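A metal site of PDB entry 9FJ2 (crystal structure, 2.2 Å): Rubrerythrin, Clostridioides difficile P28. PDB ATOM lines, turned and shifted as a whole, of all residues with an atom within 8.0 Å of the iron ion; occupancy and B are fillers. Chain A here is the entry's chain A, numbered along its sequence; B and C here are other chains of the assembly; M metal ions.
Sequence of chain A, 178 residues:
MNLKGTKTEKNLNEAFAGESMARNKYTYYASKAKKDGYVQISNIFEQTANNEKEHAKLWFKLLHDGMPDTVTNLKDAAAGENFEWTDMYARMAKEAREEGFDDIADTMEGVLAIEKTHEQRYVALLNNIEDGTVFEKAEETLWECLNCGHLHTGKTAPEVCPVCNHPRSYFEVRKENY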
ATOM      1  N   GLU A 144      -8.343 -26.162 -29.507  1.00  0.00           N
ATOM      2  CA  GLU A 144      -7.459 -26.448 -28.392  1.00  0.00           C
ATOM      3  C   GLU A 144      -6.507 -27.564 -28.778  1.00  0.00           C
ATOM      4  O   GLU A 144      -6.926 -28.576 -29.339  1.00  0.00           O
ATOM      5  CB  GLU A 144      -8.253 -26.840 -27.137  1.00  0.00           C
ATOM      6  CG  GLU A 144      -7.399 -27.461 -26.035  1.00  0.00           C
ATOM      7  CD  GLU A 144      -8.158 -27.628 -24.733  1.00  0.00           C
ATOM      8  OE1 GLU A 144      -9.257 -27.061 -24.606  1.00  0.00           O
ATOM      9  OE2 GLU A 144      -7.639 -28.324 -23.832  1.00  0.00           O
ATOM     10  N   CYS A 145      -5.216 -27.376 -28.482  1.00  0.00           N
ATOM     11  CA  CYS A 145      -4.201 -28.406 -28.718  1.00  0.00           C
ATOM     12  C   CYS A 145      -4.254 -29.406 -27.571  1.00  0.00           C
ATOM     13  O   CYS A 145      -3.942 -29.073 -26.428  1.00  0.00           O
ATOM     14  CB  CYS A 145      -2.825 -27.772 -28.841  1.00  0.00           C
ATOM     15  SG  CYS A 145      -1.463 -28.941 -29.077  1.00  0.00           S
ATOM     16  N   LEU A 146      -4.631 -30.654 -27.879  1.00  0.00           N
ATOM     17  CA  LEU A 146      -4.797 -31.677 -26.854  1.00  0.00           C
ATOM     18  C   LEU A 146      -3.480 -32.168 -26.284  1.00  0.00           C
ATOM     19  O   LEU A 146      -3.492 -33.066 -25.426  1.00  0.00           O
ATOM     20  CB  LEU A 146      -5.593 -32.854 -27.429  1.00  0.00           C
ATOM     21  CG  LEU A 146      -7.076 -32.603 -27.688  1.00  0.00           C
ATOM     22  CD1 LEU A 146      -7.631 -33.611 -28.688  1.00  0.00           C
ATOM     23  CD2 LEU A 146      -7.876 -32.626 -26.398  1.00  0.00           C
ATOM     24  N   ASN A 147      -2.340 -31.631 -26.716  1.00  0.00           N
ATOM     25  CA  ASN A 147      -1.041 -32.027 -26.193  1.00  0.00           C
ATOM     26  C   ASN A 147      -0.474 -31.015 -25.200  1.00  0.00           C
ATOM     27  O   ASN A 147      -0.067 -31.382 -24.106  1.00  0.00           O
ATOM     28  CB  ASN A 147      -0.052 -32.238 -27.337  1.00  0.00           C
ATOM     29  CG  ASN A 147       1.312 -32.702 -26.858  1.00  0.00           C
ATOM     30  OD1 ASN A 147       2.254 -31.925 -26.776  1.00  0.00           O
ATOM     31  ND2 ASN A 147       1.422 -33.990 -26.532  1.00  0.00           N
ATOM     32  N   CYS A 148      -0.453 -29.725 -25.575  1.00  0.00           N
ATOM     33  CA  CYS A 148       0.125 -28.693 -24.734  1.00  0.00           C
ATOM     34  C   CYS A 148      -0.894 -27.707 -24.178  1.00  0.00           C
ATOM     35  O   CYS A 148      -0.580 -27.012 -23.196  1.00  0.00           O
ATOM     36  CB  CYS A 148       1.188 -27.906 -25.510  1.00  0.00           C
ATOM     37  SG  CYS A 148       0.515 -26.670 -26.645  1.00  0.00           S
ATOM     38  N   GLY A 149      -2.080 -27.618 -24.760  1.00  0.00           N
ATOM     39  CA  GLY A 149      -3.085 -26.691 -24.313  1.00  0.00           C
ATOM     40  C   GLY A 149      -3.132 -25.370 -25.047  1.00  0.00           C
ATOM     41  O   GLY A 149      -3.747 -24.427 -24.540  1.00  0.00           O
ATOM     42  N   HIS A 150      -2.514 -25.274 -26.220  1.00  0.00           N
ATOM     43  CA  HIS A 150      -2.522 -24.027 -26.974  1.00  0.00           C
ATOM     44  C   HIS A 150      -3.913 -23.755 -27.529  1.00  0.00           C
ATOM     45  O   HIS A 150      -4.587 -24.649 -28.045  1.00  0.00           O
ATOM     46  CB  HIS A 150      -1.509 -24.105 -28.123  1.00  0.00           C
ATOM     47  CG  HIS A 150      -1.618 -22.971 -29.098  1.00  0.00           C
ATOM     48  ND1 HIS A 150      -1.449 -21.653 -28.742  1.00  0.00           N
ATOM     49  CD2 HIS A 150      -1.880 -22.971 -30.429  1.00  0.00           C
ATOM     50  CE1 HIS A 150      -1.602 -20.885 -29.806  1.00  0.00           C
ATOM     51  NE2 HIS A 150      -1.863 -21.664 -30.846  1.00  0.00           N
ATOM     52  N   LEU A 151      -4.338 -22.500 -27.431  1.00  0.00           N
ATOM     53  CA  LEU A 151      -5.621 -22.057 -27.950  1.00  0.00           C
ATOM     54  C   LEU A 151      -5.412 -21.265 -29.230  1.00  0.00           C
ATOM     55  O   LEU A 151      -4.531 -20.405 -29.310  1.00  0.00           O
ATOM     56  CB  LEU A 151      -6.366 -21.189 -26.928  1.00  0.00           C
ATOM     57  CG  LEU A 151      -7.099 -21.953 -25.827  1.00  0.00           C
ATOM     58  CD1 LEU A 151      -7.916 -21.005 -24.959  1.00  0.00           C
ATOM     59  CD2 LEU A 151      -7.981 -23.023 -26.447  1.00  0.00           C
ATOM     60  N   VAL A 160       0.401 -27.000 -37.890  1.00  0.00           N
ATOM     61  CA  VAL A 160       1.224 -27.494 -36.788  1.00  0.00           C
ATOM     62  C   VAL A 160       1.083 -26.529 -35.629  1.00  0.00           C
ATOM     63  O   VAL A 160       1.026 -25.308 -35.826  1.00  0.00           O
ATOM     64  CB  VAL A 160       2.710 -27.648 -37.202  1.00  0.00           C
ATOM     65  CG1 VAL A 160       3.560 -28.000 -36.002  1.00  0.00           C
ATOM     66  CG2 VAL A 160       2.861 -28.698 -38.295  1.00  0.00           C
ATOM     67  N   CYS A 161       0.986 -27.075 -34.416  1.00  0.00           N
ATOM     68  CA  CYS A 161       0.836 -26.236 -33.237  1.00  0.00           C
ATOM     69  C   CYS A 161       2.042 -25.314 -33.098  1.00  0.00           C
ATOM     70  O   CYS A 161       3.191 -25.783 -33.121  1.00  0.00           O
ATOM     71  CB  CYS A 161       0.689 -27.097 -31.981  1.00  0.00           C
ATOM     72  SG  CYS A 161       0.773 -26.167 -30.442  1.00  0.00           S
ATOM     73  N   PRO A 162       1.835 -24.001 -32.954  1.00  0.00           N
ATOM     74  CA  PRO A 162       2.963 -23.064 -32.867  1.00  0.00           C
ATOM     75  C   PRO A 162       3.601 -22.960 -31.491  1.00  0.00           C
ATOM     76  O   PRO A 162       4.463 -22.091 -31.298  1.00  0.00           O
ATOM     77  CB  PRO A 162       2.319 -21.732 -33.272  1.00  0.00           C
ATOM     78  CG  PRO A 162       0.900 -21.847 -32.827  1.00  0.00           C
ATOM     79  CD  PRO A 162       0.534 -23.319 -32.861  1.00  0.00           C
ATOM     80  N   VAL A 163       3.215 -23.803 -30.547  1.00  0.00           N
ATOM     81  CA  VAL A 163       3.800 -23.812 -29.204  1.00  0.00           C
ATOM     82  C   VAL A 163       4.634 -25.062 -28.967  1.00  0.00           C
ATOM     83  O   VAL A 163       5.828 -24.976 -28.675  1.00  0.00           O
ATOM     84  CB  VAL A 163       2.694 -23.662 -28.121  1.00  0.00           C
ATOM     85  CG1 VAL A 163       3.303 -23.784 -26.729  1.00  0.00           C
ATOM     86  CG2 VAL A 163       1.984 -22.325 -28.275  1.00  0.00           C
ATOM     87  N   CYS A 164       4.029 -26.246 -29.099  1.00  0.00           N
ATOM     88  CA  CYS A 164       4.703 -27.511 -28.853  1.00  0.00           C
ATOM     89  C   CYS A 164       5.102 -28.233 -30.134  1.00  0.00           C
ATOM     90  O   CYS A 164       5.742 -29.283 -30.064  1.00  0.00           O
ATOM     91  CB  CYS A 164       3.824 -28.425 -28.006  1.00  0.00           C
ATOM     92  SG  CYS A 164       2.295 -28.939 -28.814  1.00  0.00           S
ATOM     93  N   ASN A 165       4.716 -27.700 -31.307  1.00  0.00           N
ATOM     94  CA  ASN A 165       5.091 -28.263 -32.607  1.00  0.00           C
ATOM     95  C   ASN A 165       4.502 -29.657 -32.794  1.00  0.00           C
ATOM     96  O   ASN A 165       5.182 -30.595 -33.223  1.00  0.00           O
ATOM     97  CB  ASN A 165       6.610 -28.272 -32.787  1.00  0.00           C
ATOM     98  CG  ASN A 165       7.027 -28.261 -34.250  1.00  0.00           C
ATOM     99  OD1 ASN A 165       7.818 -29.104 -34.681  1.00  0.00           O
ATOM    100  ND2 ASN A 165       6.501 -27.314 -35.011  1.00  0.00           N
ATOM    101  N   HIS A 166       3.222 -29.806 -32.467  1.00  0.00           N
ATOM    102  CA  HIS A 166       2.490 -31.039 -32.714  1.00  0.00           C
ATOM    103  C   HIS A 166       1.525 -30.865 -33.880  1.00  0.00           C
ATOM    104  O   HIS A 166       1.028 -29.756 -34.119  1.00  0.00           O
ATOM    105  CB  HIS A 166       1.712 -31.478 -31.465  1.00  0.00           C
ATOM    106  CG  HIS A 166       2.522 -32.314 -30.516  1.00  0.00           C
ATOM    107  ND1 HIS A 166       3.639 -31.831 -29.868  1.00  0.00           N
ATOM    108  CD2 HIS A 166       2.377 -33.585 -30.102  1.00  0.00           C
ATOM    109  CE1 HIS A 166       4.151 -32.772 -29.100  1.00  0.00           C
ATOM    110  NE2 HIS A 166       3.392 -33.855 -29.222  1.00  0.00           N
ATOM    111  N   PRO A 167       1.242 -31.929 -34.653  1.00  0.00           N
ATOM    112  CA  PRO A 167       0.396 -31.774 -35.839  1.00  0.00           C
ATOM    113  C   PRO A 167      -1.062 -31.462 -35.513  1.00  0.00           C
ATOM    114  O   PRO A 167      -1.437 -31.330 -34.352  1.00  0.00           O
ATOM    115  CB  PRO A 167       0.523 -33.139 -36.531  1.00  0.00           C
ATOM    116  CG  PRO A 167       0.914 -34.087 -35.453  1.00  0.00           C
ATOM    117  CD  PRO A 167       1.769 -33.299 -34.505  1.00  0.00           C
ATOM    118  N   TYR A 170      -3.812 -33.363 -32.900  1.00  0.00           N
ATOM    119  CA  TYR A 170      -4.034 -33.018 -31.505  1.00  0.00           C
ATOM    120  C   TYR A 170      -4.944 -31.804 -31.316  1.00  0.00           C
ATOM    121  O   TYR A 170      -5.039 -31.300 -30.190  1.00  0.00           O
ATOM    122  CB  TYR A 170      -2.685 -32.756 -30.813  1.00  0.00           C
ATOM    123  CG  TYR A 170      -1.806 -33.983 -30.699  1.00  0.00           C
ATOM    124  CD1 TYR A 170      -1.077 -34.434 -31.794  1.00  0.00           C
ATOM    125  CD2 TYR A 170      -1.708 -34.682 -29.505  1.00  0.00           C
ATOM    126  CE1 TYR A 170      -0.270 -35.557 -31.690  1.00  0.00           C
ATOM    127  CE2 TYR A 170      -0.904 -35.796 -29.403  1.00  0.00           C
ATOM    128  CZ  TYR A 170      -0.193 -36.231 -30.492  1.00  0.00           C
ATOM    129  OH  TYR A 170       0.614 -37.345 -30.399  1.00  0.00           O
ATOM    130  N   PHE A 171      -5.603 -31.330 -32.365  1.00  0.00           N
ATOM    131  CA  PHE A 171      -6.468 -30.153 -32.267  1.00  0.00           C
ATOM    132  C   PHE A 171      -7.929 -30.574 -32.283  1.00  0.00           C
ATOM    133  O   PHE A 171      -8.326 -31.481 -33.016  1.00  0.00           O
ATOM    134  CB  PHE A 171      -6.188 -29.181 -33.417  1.00  0.00           C
ATOM    135  CG  PHE A 171      -5.029 -28.273 -33.167  1.00  0.00           C
ATOM    136  CD1 PHE A 171      -5.144 -27.219 -32.261  1.00  0.00           C
ATOM    137  CD2 PHE A 171      -3.828 -28.460 -33.821  1.00  0.00           C
ATOM    138  CE1 PHE A 171      -4.069 -26.378 -32.021  1.00  0.00           C
ATOM    139  CE2 PHE A 171      -2.753 -27.609 -33.592  1.00  0.00           C
ATOM    140  CZ  PHE A 171      -2.872 -26.578 -32.686  1.00  0.00           C
ATOM    141  N   ILE B 114      -1.076 -19.875 -22.289  1.00  0.00           N
ATOM    142  CA  ILE B 114      -1.783 -21.069 -21.848  1.00  0.00           C
ATOM    143  C   ILE B 114      -2.037 -21.016 -20.343  1.00  0.00           C
ATOM    144  O   ILE B 114      -3.119 -21.365 -19.868  1.00  0.00           O
ATOM    145  CB  ILE B 114      -0.999 -22.329 -22.244  1.00  0.00           C
ATOM    146  CG1 ILE B 114      -0.922 -22.456 -23.763  1.00  0.00           C
ATOM    147  CG2 ILE B 114      -1.623 -23.577 -21.636  1.00  0.00           C
ATOM    148  CD1 ILE B 114       0.022 -23.540 -24.244  1.00  0.00           C
ATOM    149  N   ASN C  51      -0.622 -31.049 -19.479  1.00  0.00           N
ATOM    150  CA  ASN C  51      -0.261 -29.836 -20.197  1.00  0.00           C
ATOM    151  C   ASN C  51       1.062 -29.274 -19.692  1.00  0.00           C
ATOM    152  O   ASN C  51       1.938 -28.910 -20.481  1.00  0.00           O
ATOM    153  CB  ASN C  51      -1.375 -28.791 -20.060  1.00  0.00           C
ATOM    154  CG  ASN C  51      -2.492 -28.991 -21.054  1.00  0.00           C
ATOM    155  OD1 ASN C  51      -2.368 -29.764 -22.003  1.00  0.00           O
ATOM    156  ND2 ASN C  51      -3.599 -28.294 -20.848  1.00  0.00           N
ATOM    157  N   GLU C  54       4.109 -31.271 -20.911  1.00  0.00           N
ATOM    158  CA  GLU C  54       4.634 -30.965 -22.235  1.00  0.00           C
ATOM    159  C   GLU C  54       5.347 -29.617 -22.264  1.00  0.00           C
ATOM    160  O   GLU C  54       6.273 -29.428 -23.067  1.00  0.00           O
ATOM    161  CB  GLU C  54       3.511 -30.982 -23.264  1.00  0.00           C
ATOM    162  CG  GLU C  54       2.911 -32.364 -23.506  1.00  0.00           C
ATOM    163  CD  GLU C  54       3.891 -33.327 -24.145  1.00  0.00           C
ATOM    164  OE1 GLU C  54       4.668 -32.885 -25.022  1.00  0.00           O
ATOM    165  OE2 GLU C  54       3.875 -34.523 -23.781  1.00  0.00           O
ATOM    166  N   HIS C  55       4.936 -28.667 -21.423  1.00  0.00           N
ATOM    167  CA  HIS C  55       5.643 -27.394 -21.338  1.00  0.00           C
ATOM    168  C   HIS C  55       7.067 -27.588 -20.837  1.00  0.00           C
ATOM    169  O   HIS C  55       8.002 -26.938 -21.324  1.00  0.00           O
ATOM    170  CB  HIS C  55       4.895 -26.422 -20.432  1.00  0.00           C
ATOM    171  CG  HIS C  55       3.521 -26.065 -20.911  1.00  0.00           C
ATOM    172  ND1 HIS C  55       2.558 -25.541 -20.086  1.00  0.00           N
ATOM    173  CD2 HIS C  55       2.960 -26.155 -22.143  1.00  0.00           C
ATOM    174  CE1 HIS C  55       1.448 -25.325 -20.784  1.00  0.00           C
ATOM    175  NE2 HIS C  55       1.670 -25.688 -22.034  1.00  0.00           N
ATOM    176  N   LEU C  58       9.447 -28.852 -23.555  1.00  0.00           N
ATOM    177  CA  LEU C  58       9.985 -27.822 -24.441  1.00  0.00           C
ATOM    178  C   LEU C  58      11.275 -27.243 -23.873  1.00  0.00           C
ATOM    179  O   LEU C  58      12.286 -27.134 -24.570  1.00  0.00           O
ATOM    180  CB  LEU C  58       8.946 -26.724 -24.657  1.00  0.00           C
ATOM    181  CG  LEU C  58       7.684 -27.125 -25.428  1.00  0.00           C
ATOM    182  CD1 LEU C  58       6.745 -25.938 -25.557  1.00  0.00           C
ATOM    183  CD2 LEU C  58       8.040 -27.679 -26.795  1.00  0.00           C
HETATM  184 FE    FE M   1       0.385 -27.631 -28.724  1.00  0.00          FE
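The side-chain sulfur (SG) of Cys 161 sits close to the backbone NH (N) of Val 163, 3.4 Å away. The backbone NH of Cys 161 lies within hydrogen-bond range of the backbone carbonyl oxygen of His 166 (2.7 Å). The backbone NH (N) of Cys 145 lies within hydrogen-bond range of the backbone carbonyl oxygen (O) of His 150 (2.8 Å). The side-chain sulfur (SG) of Cys 148 sits close to the backbone NH (N) of His 150 (3.4 Å). O of Cys 148 lies within hydrogen-bond range of NE2 of His 55 of chain C (2.9 Å). The backbone carbonyl oxygen (O) of Cys 148 sits close to the side-chain amide oxygen (OD1) of Asn 51 of chain C, at 3.5 Å. The side-chain sulfur (SG) of Cys 164 sits close to the side-chain amide oxygen (OD1) of Asn 147, 3.6 Å away. A ring nitrogen (ND1) of His 166 is in hydrogen-bond range of the backbone carbonyl oxygen of Cys 164 (3.3 Å).
Within 4 Å of the iron ion: Cys 145, Cys 148, Cys 161 and Cys 164. The nearest printed residue that does not touch the iron ion is His 150 (4.05 Å).
The iron ion is bound by SG of Cys 161, SG of Cys 145, SG of Cys 148 and SG of Cys 164. The iron ion has four donor atoms within binding distance.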
